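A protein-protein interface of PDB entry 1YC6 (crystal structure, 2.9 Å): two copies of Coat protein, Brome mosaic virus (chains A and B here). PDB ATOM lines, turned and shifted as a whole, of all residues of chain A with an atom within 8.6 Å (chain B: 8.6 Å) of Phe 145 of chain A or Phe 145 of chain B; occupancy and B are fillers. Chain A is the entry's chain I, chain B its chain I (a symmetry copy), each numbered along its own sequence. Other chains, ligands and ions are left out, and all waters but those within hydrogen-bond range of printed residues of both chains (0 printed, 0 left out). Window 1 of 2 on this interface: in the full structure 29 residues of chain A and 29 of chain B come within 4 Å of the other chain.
N of Ala 10 of chain A is in hydrogen-bond range of O of Asp 147 of chain B, 2.7 Å away. The backbone NH (N) of Ile 16 of chain A sits at hydrogen-bond distance from the backbone carbonyl oxygen (O) of Asp 146 of chain B (2.9 Å). NZ of Lys 18 of chain A is in salt-bridge range of OD1 of Asp 146 of chain B (3.1 Å). The backbone carbonyl oxygen of Phe 148 of chain B lies within hydrogen-bond range of the side-chain amino group of Lys 18 of chain A (2.9 Å). NH2 of Arg 142 of chain A is in salt-bridge range of OD1 of Asp 147 of chain B (3.998 Å). The backbone carbonyl oxygen (O) of Asp 146 of chain A is in hydrogen-bond range of the backbone NH (N) of Ile 16 of chain B (2.9 Å). The side-chain amino group (NZ) of Lys 18 of chain B lies within salt-bridge range of the side-chain carboxylate (OD1) of Asp 146 of chain A (3.1 Å). O of Asp 147 of chain A sits at hydrogen-bond distance from N of Ala 10 of chain B, 2.7 Å away. OD1 of Asp 147 of chain A lies within salt-bridge range of NH2 of Arg 142 of chain B (3.999 Å). O of Phe 148 of chain A is in hydrogen-bond range of NZ of Lys 18 of chain B (2.9 Å).
Phe 145 of chain A touches three residues of chain B. Of chain A, only Ser 15, Arg 142 and Phe 145 come within 4 Å of Phe 145 of chain B. No residue of chain A comes within 4 Å of Thr 144 of chain B. Of the printed residues of chain B, Ala 10 of chain A touches Asp 147. Of the printed residues of chain A, Phe 148 of chain B touches Ile 16 and Lys 18. Of the printed residues of chain A, Ile 16 of chain B touches Asp 146 (2.9 Å), Asp 147 (3.97 Å) and Phe 148 (3.6 Å). Of the printed residues of chain B, Ile 16 of chain A touches Asp 146 (2.9 Å), Asp 147 (3.97 Å) and Phe 148 (3.6 Å). The nearest residue of chain B that does not touch Phe 145 of chain A is Pro 143 of chain B (4.9 Å). The nearest residue of chain A that does not touch Phe 145 of chain B is Pro 143 of chain A (4.9 Å).
The backbone carbonyl oxygen of Tyr 14 of chain A sits at hydrogen-bond distance from the guanidinium group of Arg 142 of chain A (3.1 Å). O of Gly 13 of chain B sits at hydrogen-bond distance from N of Arg 142 of chain B, 2.9 Å away. The backbone NH (N) of Phe 148 of chain B lies within hydrogen-bond range of the side-chain carboxylate (OD2) of Asp 146 of chain B, at 3.4 Å.
Of the 18 printed residues of chain A, 10 touch a printed residue of chain B. Hydrophobic or aromatic side chains of chain A that line the printed part of chain B: Ala 10, Ile 16 and Phe 145. Hydrophobic or aromatic side chains of chain B within 4 Å of the printed part of chain A: Ala 10, Ile 16 and Phe 145. Among the printed residues, 23 pairs touch across the chains. Among the printed residues, Asp or Glu carboxylates within 4 Å of a Lys or Arg side-chain nitrogen of the other chain: Lys 18 of chain A with Asp 146 of chain B (3.1 Å), Arg 142 of chain A with Asp 147 of chain B (3.998 Å), Asp 146 of chain A with Lys 18 of chain B (3.1 Å) and Asp 147 of chain A with Arg 142 of chain B (3.999 Å).
Arg 142 of chain A touches Phe 145 of chain B, and with the chains exchanged Phe 145 of chain A touches Arg 142 of chain B. Arg 142 of chain A touches Asp 147 of chain B, and with the chains exchanged Asp 147 of chain A touches Arg 142 of chain B. Phe 145 of chain A touches its own counterpart, Phe 145 of chain B.
Among the printed residues, merely in contact across the chains: Tyr 14 of chain A with Asp 147 of chain B (3.8 Å), Ser 15 of chain A with Phe 145 of chain B (3.6 Å), Ser 15 of chain A with Asp 146 of chain B (3.6 Å), Ile 16 of chain A with Asp 147 of chain B (3.97 Å), Ile 16 of chain A with Phe 148 of chain B (3.6 Å), Arg 142 of chain A with Phe 145 of chain B (3.0 Å), Phe 145 of chain A with Ser 15 of chain B (3.6 Å), Phe 145 of chain A with Arg 142 of chain B (3.0 Å), Phe 145 of chain A with Phe 145 of chain B (3.3 Å), Asp 146 of chain A with Ser 15 of chain B (3.6 Å), Asp 147 of chain A with Tyr 14 of chain B (3.8 Å), Asp 147 of chain A with Ile 16 of chain B (3.97 Å) and Phe 148 of chain A with Ile 16 of chain B (3.6 Å).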
ATOM      1  N   ALA A  10      -5.308  -8.038   3.637  1.00  0.00           N
ATOM      2  CA  ALA A  10      -5.298  -6.906   2.710  1.00  0.00           C
ATOM      3  C   ALA A  10      -6.285  -5.817   3.165  1.00  0.00           C
ATOM      4  O   ALA A  10      -7.288  -6.105   3.829  1.00  0.00           O
ATOM      5  CB  ALA A  10      -5.656  -7.380   1.316  1.00  0.00           C
ATOM      6  N   GLY A  13     -10.687  -2.738  -0.387  1.00  0.00           N
ATOM      7  CA  GLY A  13     -10.591  -2.345  -1.782  1.00  0.00           C
ATOM      8  C   GLY A  13      -9.425  -2.945  -2.542  1.00  0.00           C
ATOM      9  O   GLY A  13      -9.355  -2.870  -3.785  1.00  0.00           O
ATOM     10  N   TYR A  14      -8.501  -3.545  -1.798  1.00  0.00           N
ATOM     11  CA  TYR A  14      -7.346  -4.162  -2.418  1.00  0.00           C
ATOM     12  C   TYR A  14      -7.422  -5.669  -2.336  1.00  0.00           C
ATOM     13  O   TYR A  14      -8.195  -6.239  -1.555  1.00  0.00           O
ATOM     14  CB  TYR A  14      -6.070  -3.711  -1.736  1.00  0.00           C
ATOM     15  CG  TYR A  14      -5.744  -2.247  -1.894  1.00  0.00           C
ATOM     16  CD1 TYR A  14      -6.571  -1.261  -1.352  1.00  0.00           C
ATOM     17  CD2 TYR A  14      -4.576  -1.846  -2.556  1.00  0.00           C
ATOM     18  CE1 TYR A  14      -6.243   0.089  -1.461  1.00  0.00           C
ATOM     19  CE2 TYR A  14      -4.236  -0.503  -2.673  1.00  0.00           C
ATOM     20  CZ  TYR A  14      -5.075   0.462  -2.123  1.00  0.00           C
ATOM     21  OH  TYR A  14      -4.744   1.796  -2.244  1.00  0.00           O
ATOM     22  N   SER A  15      -6.604  -6.310  -3.154  1.00  0.00           N
ATOM     23  CA  SER A  15      -6.525  -7.764  -3.190  1.00  0.00           C
ATOM     24  C   SER A  15      -5.043  -8.086  -3.365  1.00  0.00           C
ATOM     25  O   SER A  15      -4.240  -7.186  -3.579  1.00  0.00           O
ATOM     26  CB  SER A  15      -7.348  -8.317  -4.358  1.00  0.00           C
ATOM     27  OG  SER A  15      -6.828  -7.895  -5.618  1.00  0.00           O
ATOM     28  N   ILE A  16      -4.667  -9.352  -3.297  1.00  0.00           N
ATOM     29  CA  ILE A  16      -3.257  -9.684  -3.407  1.00  0.00           C
ATOM     30  C   ILE A  16      -2.915 -10.637  -4.546  1.00  0.00           C
ATOM     31  O   ILE A  16      -3.395 -11.768  -4.599  1.00  0.00           O
ATOM     32  CB  ILE A  16      -2.778 -10.267  -2.068  1.00  0.00           C
ATOM     33  CG1 ILE A  16      -2.936  -9.207  -0.990  1.00  0.00           C
ATOM     34  CG2 ILE A  16      -1.337 -10.728  -2.150  1.00  0.00           C
ATOM     35  CD1 ILE A  16      -2.745  -9.736   0.369  1.00  0.00           C
ATOM     36  N   SER A  17      -2.075 -10.171  -5.464  1.00  0.00           N
ATOM     37  CA  SER A  17      -1.655 -10.989  -6.599  1.00  0.00           C
ATOM     38  C   SER A  17      -0.329 -11.657  -6.270  1.00  0.00           C
ATOM     39  O   SER A  17       0.638 -10.998  -5.898  1.00  0.00           O
ATOM     40  CB  SER A  17      -1.494 -10.120  -7.850  1.00  0.00           C
ATOM     41  OG  SER A  17      -2.722  -9.510  -8.212  1.00  0.00           O
ATOM     42  N   LYS A  18      -0.270 -12.968  -6.419  1.00  0.00           N
ATOM     43  CA  LYS A  18       0.959 -13.666  -6.090  1.00  0.00           C
ATOM     44  C   LYS A  18       1.503 -14.395  -7.289  1.00  0.00           C
ATOM     45  O   LYS A  18       0.744 -14.968  -8.078  1.00  0.00           O
ATOM     46  CB  LYS A  18       0.699 -14.670  -4.969  1.00  0.00           C
ATOM     47  CG  LYS A  18      -0.253 -14.145  -3.893  1.00  0.00           C
ATOM     48  CD  LYS A  18      -0.415 -15.131  -2.757  1.00  0.00           C
ATOM     49  CE  LYS A  18      -1.381 -14.606  -1.694  1.00  0.00           C
ATOM     50  NZ  LYS A  18      -1.518 -15.554  -0.535  1.00  0.00           N
ATOM     51  N   LYS A  46      -5.360  -0.745 -18.579  1.00  0.00           N
ATOM     52  CA  LYS A  46      -6.307  -0.440 -17.517  1.00  0.00           C
ATOM     53  C   LYS A  46      -5.728  -0.871 -16.160  1.00  0.00           C
ATOM     54  O   LYS A  46      -5.846  -0.149 -15.161  1.00  0.00           O
ATOM     55  CB  LYS A  46      -7.625  -1.177 -17.798  1.00  0.00           C
ATOM     56  CG  LYS A  46      -8.755  -0.914 -16.807  1.00  0.00           C
ATOM     57  CD  LYS A  46      -9.258   0.519 -16.904  1.00  0.00           C
ATOM     58  CE  LYS A  46     -10.437   0.762 -15.965  1.00  0.00           C
ATOM     59  NZ  LYS A  46     -10.936   2.168 -16.055  1.00  0.00           N
ATOM     60  N   ASN A  47      -5.086  -2.039 -16.141  1.00  0.00           N
ATOM     61  CA  ASN A  47      -4.512  -2.587 -14.914  1.00  0.00           C
ATOM     62  C   ASN A  47      -3.150  -2.036 -14.511  1.00  0.00           C
ATOM     63  O   ASN A  47      -2.922  -1.766 -13.329  1.00  0.00           O
ATOM     64  CB  ASN A  47      -4.417  -4.115 -14.992  1.00  0.00           C
ATOM     65  CG  ASN A  47      -5.780  -4.792 -14.998  1.00  0.00           C
ATOM     66  OD1 ASN A  47      -6.738  -4.330 -14.361  1.00  0.00           O
ATOM     67  ND2 ASN A  47      -5.868  -5.907 -15.707  1.00  0.00           N
ATOM     68  N   HIS A 140      -2.598  -4.728  -4.257  1.00  0.00           N
ATOM     69  CA  HIS A 140      -2.914  -3.594  -5.119  1.00  0.00           C
ATOM     70  C   HIS A 140      -4.402  -3.383  -5.189  1.00  0.00           C
ATOM     71  O   HIS A 140      -5.183  -4.227  -4.728  1.00  0.00           O
ATOM     72  CB  HIS A 140      -2.370  -3.829  -6.522  1.00  0.00           C
ATOM     73  CG  HIS A 140      -2.892  -5.070  -7.160  1.00  0.00           C
ATOM     74  ND1 HIS A 140      -4.208  -5.208  -7.540  1.00  0.00           N
ATOM     75  CD2 HIS A 140      -2.282  -6.239  -7.463  1.00  0.00           C
ATOM     76  CE1 HIS A 140      -4.386  -6.412  -8.053  1.00  0.00           C
ATOM     77  NE2 HIS A 140      -3.232  -7.058  -8.017  1.00  0.00           N
ATOM     78  N   VAL A 141      -4.798  -2.250  -5.754  1.00  0.00           N
ATOM     79  CA  VAL A 141      -6.210  -1.958  -5.875  1.00  0.00           C
ATOM     80  C   VAL A 141      -6.841  -3.021  -6.738  1.00  0.00           C
ATOM     81  O   VAL A 141      -6.290  -3.427  -7.767  1.00  0.00           O
ATOM     82  CB  VAL A 141      -6.466  -0.607  -6.501  1.00  0.00           C
ATOM     83  CG1 VAL A 141      -7.964  -0.407  -6.644  1.00  0.00           C
ATOM     84  CG2 VAL A 141      -5.863   0.484  -5.630  1.00  0.00           C
ATOM     85  N   ARG A 142      -8.007  -3.464  -6.289  1.00  0.00           N
ATOM     86  CA  ARG A 142      -8.751  -4.507  -6.957  1.00  0.00           C
ATOM     87  C   ARG A 142      -9.134  -4.123  -8.366  1.00  0.00           C
ATOM     88  O   ARG A 142      -9.845  -3.129  -8.600  1.00  0.00           O
ATOM     89  CB  ARG A 142      -9.991  -4.842  -6.144  1.00  0.00           C
ATOM     90  CG  ARG A 142     -10.492  -6.248  -6.342  1.00  0.00           C
ATOM     91  CD  ARG A 142     -11.565  -6.501  -5.319  1.00  0.00           C
ATOM     92  NE  ARG A 142     -11.057  -6.347  -3.956  1.00  0.00           N
ATOM     93  CZ  ARG A 142     -11.785  -6.557  -2.861  1.00  0.00           C
ATOM     94  NH1 ARG A 142     -13.056  -6.932  -2.970  1.00  0.00           N
ATOM     95  NH2 ARG A 142     -11.244  -6.390  -1.656  1.00  0.00           N
ATOM     96  N   PRO A 143      -8.644  -4.913  -9.329  1.00  0.00           N
ATOM     97  CA  PRO A 143      -8.961  -4.626 -10.722  1.00  0.00           C
ATOM     98  C   PRO A 143     -10.467  -4.690 -10.812  1.00  0.00           C
ATOM     99  O   PRO A 143     -11.105  -5.477 -10.104  1.00  0.00           O
ATOM    100  CB  PRO A 143      -8.269  -5.758 -11.475  1.00  0.00           C
ATOM    101  CG  PRO A 143      -8.328  -6.894 -10.496  1.00  0.00           C
ATOM    102  CD  PRO A 143      -7.993  -6.229  -9.184  1.00  0.00           C
ATOM    103  N   THR A 144     -11.041  -3.829 -11.642  1.00  0.00           N
ATOM    104  CA  THR A 144     -12.491  -3.809 -11.822  1.00  0.00           C
ATOM    105  C   THR A 144     -12.873  -4.751 -12.952  1.00  0.00           C
ATOM    106  O   THR A 144     -12.117  -4.934 -13.922  1.00  0.00           O
ATOM    107  CB  THR A 144     -13.028  -2.400 -12.171  1.00  0.00           C
ATOM    108  OG1 THR A 144     -12.138  -1.770 -13.104  1.00  0.00           O
ATOM    109  CG2 THR A 144     -13.175  -1.543 -10.916  1.00  0.00           C
ATOM    110  N   PHE A 145     -14.052  -5.347 -12.811  1.00  0.00           N
ATOM    111  CA  PHE A 145     -14.562  -6.286 -13.805  1.00  0.00           C
ATOM    112  C   PHE A 145     -15.711  -5.674 -14.581  1.00  0.00           C
ATOM    113  O   PHE A 145     -16.417  -4.786 -14.092  1.00  0.00           O
ATOM    114  CB  PHE A 145     -15.028  -7.599 -13.148  1.00  0.00           C
ATOM    115  CG  PHE A 145     -14.936  -7.597 -11.646  1.00  0.00           C
ATOM    116  CD1 PHE A 145     -15.627  -6.634 -10.897  1.00  0.00           C
ATOM    117  CD2 PHE A 145     -14.111  -8.518 -10.982  1.00  0.00           C
ATOM    118  CE1 PHE A 145     -15.491  -6.579  -9.507  1.00  0.00           C
ATOM    119  CE2 PHE A 145     -13.964  -8.478  -9.591  1.00  0.00           C
ATOM    120  CZ  PHE A 145     -14.653  -7.505  -8.847  1.00  0.00           C
ATOM    121  N   ASP A 146     -15.879  -6.168 -15.799  1.00  0.00           N
ATOM    122  CA  ASP A 146     -16.914  -5.719 -16.705  1.00  0.00           C
ATOM    123  C   ASP A 146     -18.292  -6.043 -16.150  1.00  0.00           C
ATOM    124  O   ASP A 146     -18.555  -7.174 -15.763  1.00  0.00           O
ATOM    125  CB  ASP A 146     -16.707  -6.415 -18.039  1.00  0.00           C
ATOM    126  CG  ASP A 146     -17.020  -5.523 -19.211  1.00  0.00           C
ATOM    127  OD1 ASP A 146     -16.372  -5.717 -20.268  1.00  0.00           O
ATOM    128  OD2 ASP A 146     -17.912  -4.640 -19.075  1.00  0.00           O
ATOM    129  N   ASP A 147     -19.174  -5.056 -16.096  1.00  0.00           N
ATOM    130  CA  ASP A 147     -20.505  -5.316 -15.579  1.00  0.00           C
ATOM    131  C   ASP A 147     -21.550  -5.209 -16.655  1.00  0.00           C
ATOM    132  O   ASP A 147     -22.749  -5.303 -16.374  1.00  0.00           O
ATOM    133  CB  ASP A 147     -20.871  -4.344 -14.464  1.00  0.00           C
ATOM    134  CG  ASP A 147     -20.053  -4.566 -13.208  1.00  0.00           C
ATOM    135  OD1 ASP A 147     -19.913  -5.753 -12.783  1.00  0.00           O
ATOM    136  OD2 ASP A 147     -19.558  -3.551 -12.645  1.00  0.00           O
ATOM    137  N   PHE A 148     -21.104  -5.005 -17.889  1.00  0.00           N
ATOM    138  CA  PHE A 148     -22.047  -4.870 -18.974  1.00  0.00           C
ATOM    139  C   PHE A 148     -21.707  -5.740 -20.151  1.00  0.00           C
ATOM    140  O   PHE A 148     -20.543  -5.938 -20.472  1.00  0.00           O
ATOM    141  CB  PHE A 148     -22.118  -3.414 -19.435  1.00  0.00           C
ATOM    142  CG  PHE A 148     -22.531  -2.455 -18.354  1.00  0.00           C
ATOM    143  CD1 PHE A 148     -21.582  -1.868 -17.521  1.00  0.00           C
ATOM    144  CD2 PHE A 148     -23.872  -2.164 -18.144  1.00  0.00           C
ATOM    145  CE1 PHE A 148     -21.966  -1.008 -16.497  1.00  0.00           C
ATOM    146  CE2 PHE A 148     -24.265  -1.301 -17.116  1.00  0.00           C
ATOM    147  CZ  PHE A 148     -23.310  -0.724 -16.295  1.00  0.00           C
ATOM    148  N   ALA B  10     -24.931  -6.690 -15.702  1.00  0.00           N
ATOM    149  CA  ALA B  10     -24.773  -7.937 -14.953  1.00  0.00           C
ATOM    150  C   ALA B  10     -25.492  -7.856 -13.596  1.00  0.00           C
ATOM    151  O   ALA B  10     -25.651  -6.770 -13.025  1.00  0.00           O
ATOM    152  CB  ALA B  10     -23.300  -8.228 -14.743  1.00  0.00           C
ATOM    153  N   GLY B  13     -23.198  -9.488  -7.804  1.00  0.00           N
ATOM    154  CA  GLY B  13     -22.287 -10.572  -7.478  1.00  0.00           C
ATOM    155  C   GLY B  13     -21.619 -11.231  -8.668  1.00  0.00           C
ATOM    156  O   GLY B  13     -20.658 -12.013  -8.520  1.00  0.00           O
ATOM    157  N   TYR B  14     -22.123 -10.918  -9.858  1.00  0.00           N
ATOM    158  CA  TYR B  14     -21.557 -11.483 -11.066  1.00  0.00           C
ATOM    159  C   TYR B  14     -20.811 -10.435 -11.860  1.00  0.00           C
ATOM    160  O   TYR B  14     -20.970  -9.225 -11.650  1.00  0.00           O
ATOM    161  CB  TYR B  14     -22.646 -12.061 -11.946  1.00  0.00           C
ATOM    162  CG  TYR B  14     -23.365 -13.256 -11.371  1.00  0.00           C
ATOM    163  CD1 TYR B  14     -24.138 -13.144 -10.213  1.00  0.00           C
ATOM    164  CD2 TYR B  14     -23.305 -14.499 -12.014  1.00  0.00           C
ATOM    165  CE1 TYR B  14     -24.837 -14.240  -9.710  1.00  0.00           C
ATOM    166  CE2 TYR B  14     -23.996 -15.601 -11.523  1.00  0.00           C
ATOM    167  CZ  TYR B  14     -24.762 -15.466 -10.369  1.00  0.00           C
ATOM    168  OH  TYR B  14     -25.443 -16.559  -9.875  1.00  0.00           O
ATOM    169  N   SER B  15     -19.993 -10.916 -12.781  1.00  0.00           N
ATOM    170  CA  SER B  15     -19.214 -10.050 -13.656  1.00  0.00           C
ATOM    171  C   SER B  15     -19.242 -10.725 -15.025  1.00  0.00           C
ATOM    172  O   SER B  15     -19.728 -11.844 -15.149  1.00  0.00           O
ATOM    173  CB  SER B  15     -17.778  -9.918 -13.140  1.00  0.00           C
ATOM    174  OG  SER B  15     -17.090 -11.168 -13.163  1.00  0.00           O
ATOM    175  N   ILE B  16     -18.716 -10.078 -16.051  1.00  0.00           N
ATOM    176  CA  ILE B  16     -18.777 -10.672 -17.376  1.00  0.00           C
ATOM    177  C   ILE B  16     -17.422 -10.884 -18.040  1.00  0.00           C
ATOM    178  O   ILE B  16     -16.671  -9.939 -18.275  1.00  0.00           O
ATOM    179  CB  ILE B  16     -19.674  -9.803 -18.270  1.00  0.00           C
ATOM    180  CG1 ILE B  16     -21.078  -9.791 -17.689  1.00  0.00           C
ATOM    181  CG2 ILE B  16     -19.696 -10.315 -19.696  1.00  0.00           C
ATOM    182  CD1 ILE B  16     -21.954  -8.792 -18.320  1.00  0.00           C
ATOM    183  N   SER B  17     -17.111 -12.139 -18.345  1.00  0.00           N
ATOM    184  CA  SER B  17     -15.848 -12.475 -18.998  1.00  0.00           C
ATOM    185  C   SER B  17     -16.070 -12.565 -20.500  1.00  0.00           C
ATOM    186  O   SER B  17     -16.945 -13.287 -20.969  1.00  0.00           O
ATOM    187  CB  SER B  17     -15.322 -13.816 -18.478  1.00  0.00           C
ATOM    188  OG  SER B  17     -15.064 -13.761 -17.084  1.00  0.00           O
ATOM    189  N   LYS B  18     -15.271 -11.843 -21.264  1.00  0.00           N
ATOM    190  CA  LYS B  18     -15.454 -11.862 -22.702  1.00  0.00           C
ATOM    191  C   LYS B  18     -14.215 -12.356 -23.398  1.00  0.00           C
ATOM    192  O   LYS B  18     -13.092 -12.033 -22.995  1.00  0.00           O
ATOM    193  CB  LYS B  18     -15.780 -10.455 -23.200  1.00  0.00           C
ATOM    194  CG  LYS B  18     -16.718  -9.684 -22.269  1.00  0.00           C
ATOM    195  CD  LYS B  18     -17.089  -8.332 -22.839  1.00  0.00           C
ATOM    196  CE  LYS B  18     -18.012  -7.562 -21.895  1.00  0.00           C
ATOM    197  NZ  LYS B  18     -18.427  -6.235 -22.466  1.00  0.00           N
ATOM    198  N   LYS B  46     -10.607 -23.773  -8.650  1.00  0.00           N
ATOM    199  CA  LYS B  46     -11.418 -22.873  -7.844  1.00  0.00           C
ATOM    200  C   LYS B  46     -12.433 -22.142  -8.738  1.00  0.00           C
ATOM    201  O   LYS B  46     -13.604 -21.980  -8.367  1.00  0.00           O
ATOM    202  CB  LYS B  46     -10.495 -21.863  -7.143  1.00  0.00           C
ATOM    203  CG  LYS B  46     -11.184 -20.879  -6.202  1.00  0.00           C
ATOM    204  CD  LYS B  46     -11.745 -21.583  -4.975  1.00  0.00           C
ATOM    205  CE  LYS B  46     -12.369 -20.589  -3.998  1.00  0.00           C
ATOM    206  NZ  LYS B  46     -12.922 -21.273  -2.790  1.00  0.00           N
ATOM    207  N   ASN B  47     -11.980 -21.725  -9.920  1.00  0.00           N
ATOM    208  CA  ASN B  47     -12.826 -20.991 -10.858  1.00  0.00           C
ATOM    209  C   ASN B  47     -13.761 -21.835 -11.715  1.00  0.00           C
ATOM    210  O   ASN B  47     -14.922 -21.464 -11.905  1.00  0.00           O
ATOM    211  CB  ASN B  47     -11.978 -20.109 -11.782  1.00  0.00           C
ATOM    212  CG  ASN B  47     -11.302 -18.961 -11.046  1.00  0.00           C
ATOM    213  OD1 ASN B  47     -11.845 -18.393 -10.088  1.00  0.00           O
ATOM    214  ND2 ASN B  47     -10.113 -18.602 -11.507  1.00  0.00           N
ATOM    215  N   HIS B 140     -20.850 -14.658 -15.023  1.00  0.00           N
ATOM    216  CA  HIS B 140     -20.671 -15.698 -14.016  1.00  0.00           C
ATOM    217  C   HIS B 140     -20.382 -15.087 -12.672  1.00  0.00           C
ATOM    218  O   HIS B 140     -20.132 -13.878 -12.568  1.00  0.00           O
ATOM    219  CB  HIS B 140     -19.525 -16.623 -14.408  1.00  0.00           C
ATOM    220  CG  HIS B 140     -18.228 -15.913 -14.594  1.00  0.00           C
ATOM    221  ND1 HIS B 140     -17.541 -15.343 -13.545  1.00  0.00           N
ATOM    222  CD2 HIS B 140     -17.504 -15.659 -15.708  1.00  0.00           C
ATOM    223  CE1 HIS B 140     -16.445 -14.769 -14.008  1.00  0.00           C
ATOM    224  NE2 HIS B 140     -16.400 -14.946 -15.317  1.00  0.00           N
ATOM    225  N   VAL B 141     -20.427 -15.918 -11.639  1.00  0.00           N
ATOM    226  CA  VAL B 141     -20.156 -15.427 -10.305  1.00  0.00           C
ATOM    227  C   VAL B 141     -18.744 -14.900 -10.272  1.00  0.00           C
ATOM    228  O   VAL B 141     -17.815 -15.508 -10.814  1.00  0.00           O
ATOM    229  CB  VAL B 141     -20.298 -16.504  -9.256  1.00  0.00           C
ATOM    230  CG1 VAL B 141     -19.942 -15.922  -7.901  1.00  0.00           C
ATOM    231  CG2 VAL B 141     -21.725 -17.030  -9.251  1.00  0.00           C
ATOM    232  N   ARG B 142     -18.608 -13.750  -9.626  1.00  0.00           N
ATOM    233  CA  ARG B 142     -17.340 -13.067  -9.515  1.00  0.00           C
ATOM    234  C   ARG B 142     -16.303 -13.899  -8.801  1.00  0.00           C
ATOM    235  O   ARG B 142     -16.472 -14.289  -7.631  1.00  0.00           O
ATOM    236  CB  ARG B 142     -17.542 -11.742  -8.796  1.00  0.00           C
ATOM    237  CG  ARG B 142     -16.523 -10.692  -9.149  1.00  0.00           C
ATOM    238  CD  ARG B 142     -16.978  -9.390  -8.548  1.00  0.00           C
ATOM    239  NE  ARG B 142     -18.290  -8.993  -9.056  1.00  0.00           N
ATOM    240  CZ  ARG B 142     -18.907  -7.860  -8.723  1.00  0.00           C
ATOM    241  NH1 ARG B 142     -18.326  -7.011  -7.880  1.00  0.00           N
ATOM    242  NH2 ARG B 142     -20.105  -7.576  -9.229  1.00  0.00           N
ATOM    243  N   PRO B 143     -15.211 -14.194  -9.518  1.00  0.00           N
ATOM    244  CA  PRO B 143     -14.151 -14.991  -8.915  1.00  0.00           C
ATOM    245  C   PRO B 143     -13.697 -14.205  -7.708  1.00  0.00           C
ATOM    246  O   PRO B 143     -13.713 -12.970  -7.721  1.00  0.00           O
ATOM    247  CB  PRO B 143     -13.098 -15.056 -10.017  1.00  0.00           C
ATOM    248  CG  PRO B 143     -13.285 -13.751 -10.734  1.00  0.00           C
ATOM    249  CD  PRO B 143     -14.785 -13.617 -10.807  1.00  0.00           C
ATOM    250  N   THR B 144     -13.340 -14.917  -6.647  1.00  0.00           N
ATOM    251  CA  THR B 144     -12.869 -14.265  -5.427  1.00  0.00           C
ATOM    252  C   THR B 144     -11.360 -14.097  -5.494  1.00  0.00           C
ATOM    253  O   THR B 144     -10.645 -14.923  -6.087  1.00  0.00           O
ATOM    254  CB  THR B 144     -13.204 -15.077  -4.151  1.00  0.00           C
ATOM    255  OG1 THR B 144     -12.978 -16.471  -4.403  1.00  0.00           O
ATOM    256  CG2 THR B 144     -14.648 -14.842  -3.716  1.00  0.00           C
ATOM    257  N   PHE B 145     -10.888 -13.015  -4.883  1.00  0.00           N
ATOM    258  CA  PHE B 145      -9.463 -12.705  -4.862  1.00  0.00           C
ATOM    259  C   PHE B 145      -8.887 -12.924  -3.477  1.00  0.00           C
ATOM    260  O   PHE B 145      -9.593 -12.843  -2.466  1.00  0.00           O
ATOM    261  CB  PHE B 145      -9.199 -11.252  -5.304  1.00  0.00           C
ATOM    262  CG  PHE B 145     -10.450 -10.460  -5.576  1.00  0.00           C
ATOM    263  CD1 PHE B 145     -11.411 -10.289  -4.569  1.00  0.00           C
ATOM    264  CD2 PHE B 145     -10.697  -9.935  -6.854  1.00  0.00           C
ATOM    265  CE1 PHE B 145     -12.607  -9.617  -4.831  1.00  0.00           C
ATOM    266  CE2 PHE B 145     -11.889  -9.258  -7.134  1.00  0.00           C
ATOM    267  CZ  PHE B 145     -12.852  -9.099  -6.123  1.00  0.00           C
ATOM    268  N   ASP B 146      -7.592 -13.203  -3.457  1.00  0.00           N
ATOM    269  CA  ASP B 146      -6.849 -13.451  -2.240  1.00  0.00           C
ATOM    270  C   ASP B 146      -6.815 -12.206  -1.368  1.00  0.00           C
ATOM    271  O   ASP B 146      -6.473 -11.129  -1.839  1.00  0.00           O
ATOM    272  CB  ASP B 146      -5.439 -13.864  -2.624  1.00  0.00           C
ATOM    273  CG  ASP B 146      -4.880 -14.925  -1.714  1.00  0.00           C
ATOM    274  OD1 ASP B 146      -4.063 -15.736  -2.213  1.00  0.00           O
ATOM    275  OD2 ASP B 146      -5.251 -14.941  -0.508  1.00  0.00           O
ATOM    276  N   ASP B 147      -7.176 -12.340  -0.101  1.00  0.00           N
ATOM    277  CA  ASP B 147      -7.155 -11.181   0.773  1.00  0.00           C
ATOM    278  C   ASP B 147      -6.090 -11.302   1.829  1.00  0.00           C
ATOM    279  O   ASP B 147      -5.994 -10.451   2.719  1.00  0.00           O
ATOM    280  CB  ASP B 147      -8.495 -10.983   1.471  1.00  0.00           C
ATOM    281  CG  ASP B 147      -9.592 -10.569   0.513  1.00  0.00           C
ATOM    282  OD1 ASP B 147      -9.346  -9.647  -0.323  1.00  0.00           O
ATOM    283  OD2 ASP B 147     -10.703 -11.162   0.603  1.00  0.00           O
ATOM    284  N   PHE B 148      -5.292 -12.359   1.741  1.00  0.00           N
ATOM    285  CA  PHE B 148      -4.258 -12.556   2.730  1.00  0.00           C
ATOM    286  C   PHE B 148      -2.916 -12.840   2.119  1.00  0.00           C
ATOM    287  O   PHE B 148      -2.817 -13.508   1.099  1.00  0.00           O
ATOM    288  CB  PHE B 148      -4.634 -13.706   3.665  1.00  0.00           C
ATOM    289  CG  PHE B 148      -5.929 -13.493   4.399  1.00  0.00           C
ATOM    290  CD1 PHE B 148      -7.138 -13.902   3.843  1.00  0.00           C
ATOM    291  CD2 PHE B 148      -5.945 -12.853   5.630  1.00  0.00           C
ATOM    292  CE1 PHE B 148      -8.341 -13.673   4.504  1.00  0.00           C
ATOM    293  CE2 PHE B 148      -7.150 -12.620   6.301  1.00  0.00           C
ATOM    294  CZ  PHE B 148      -8.345 -13.032   5.735  1.00  0.00           C
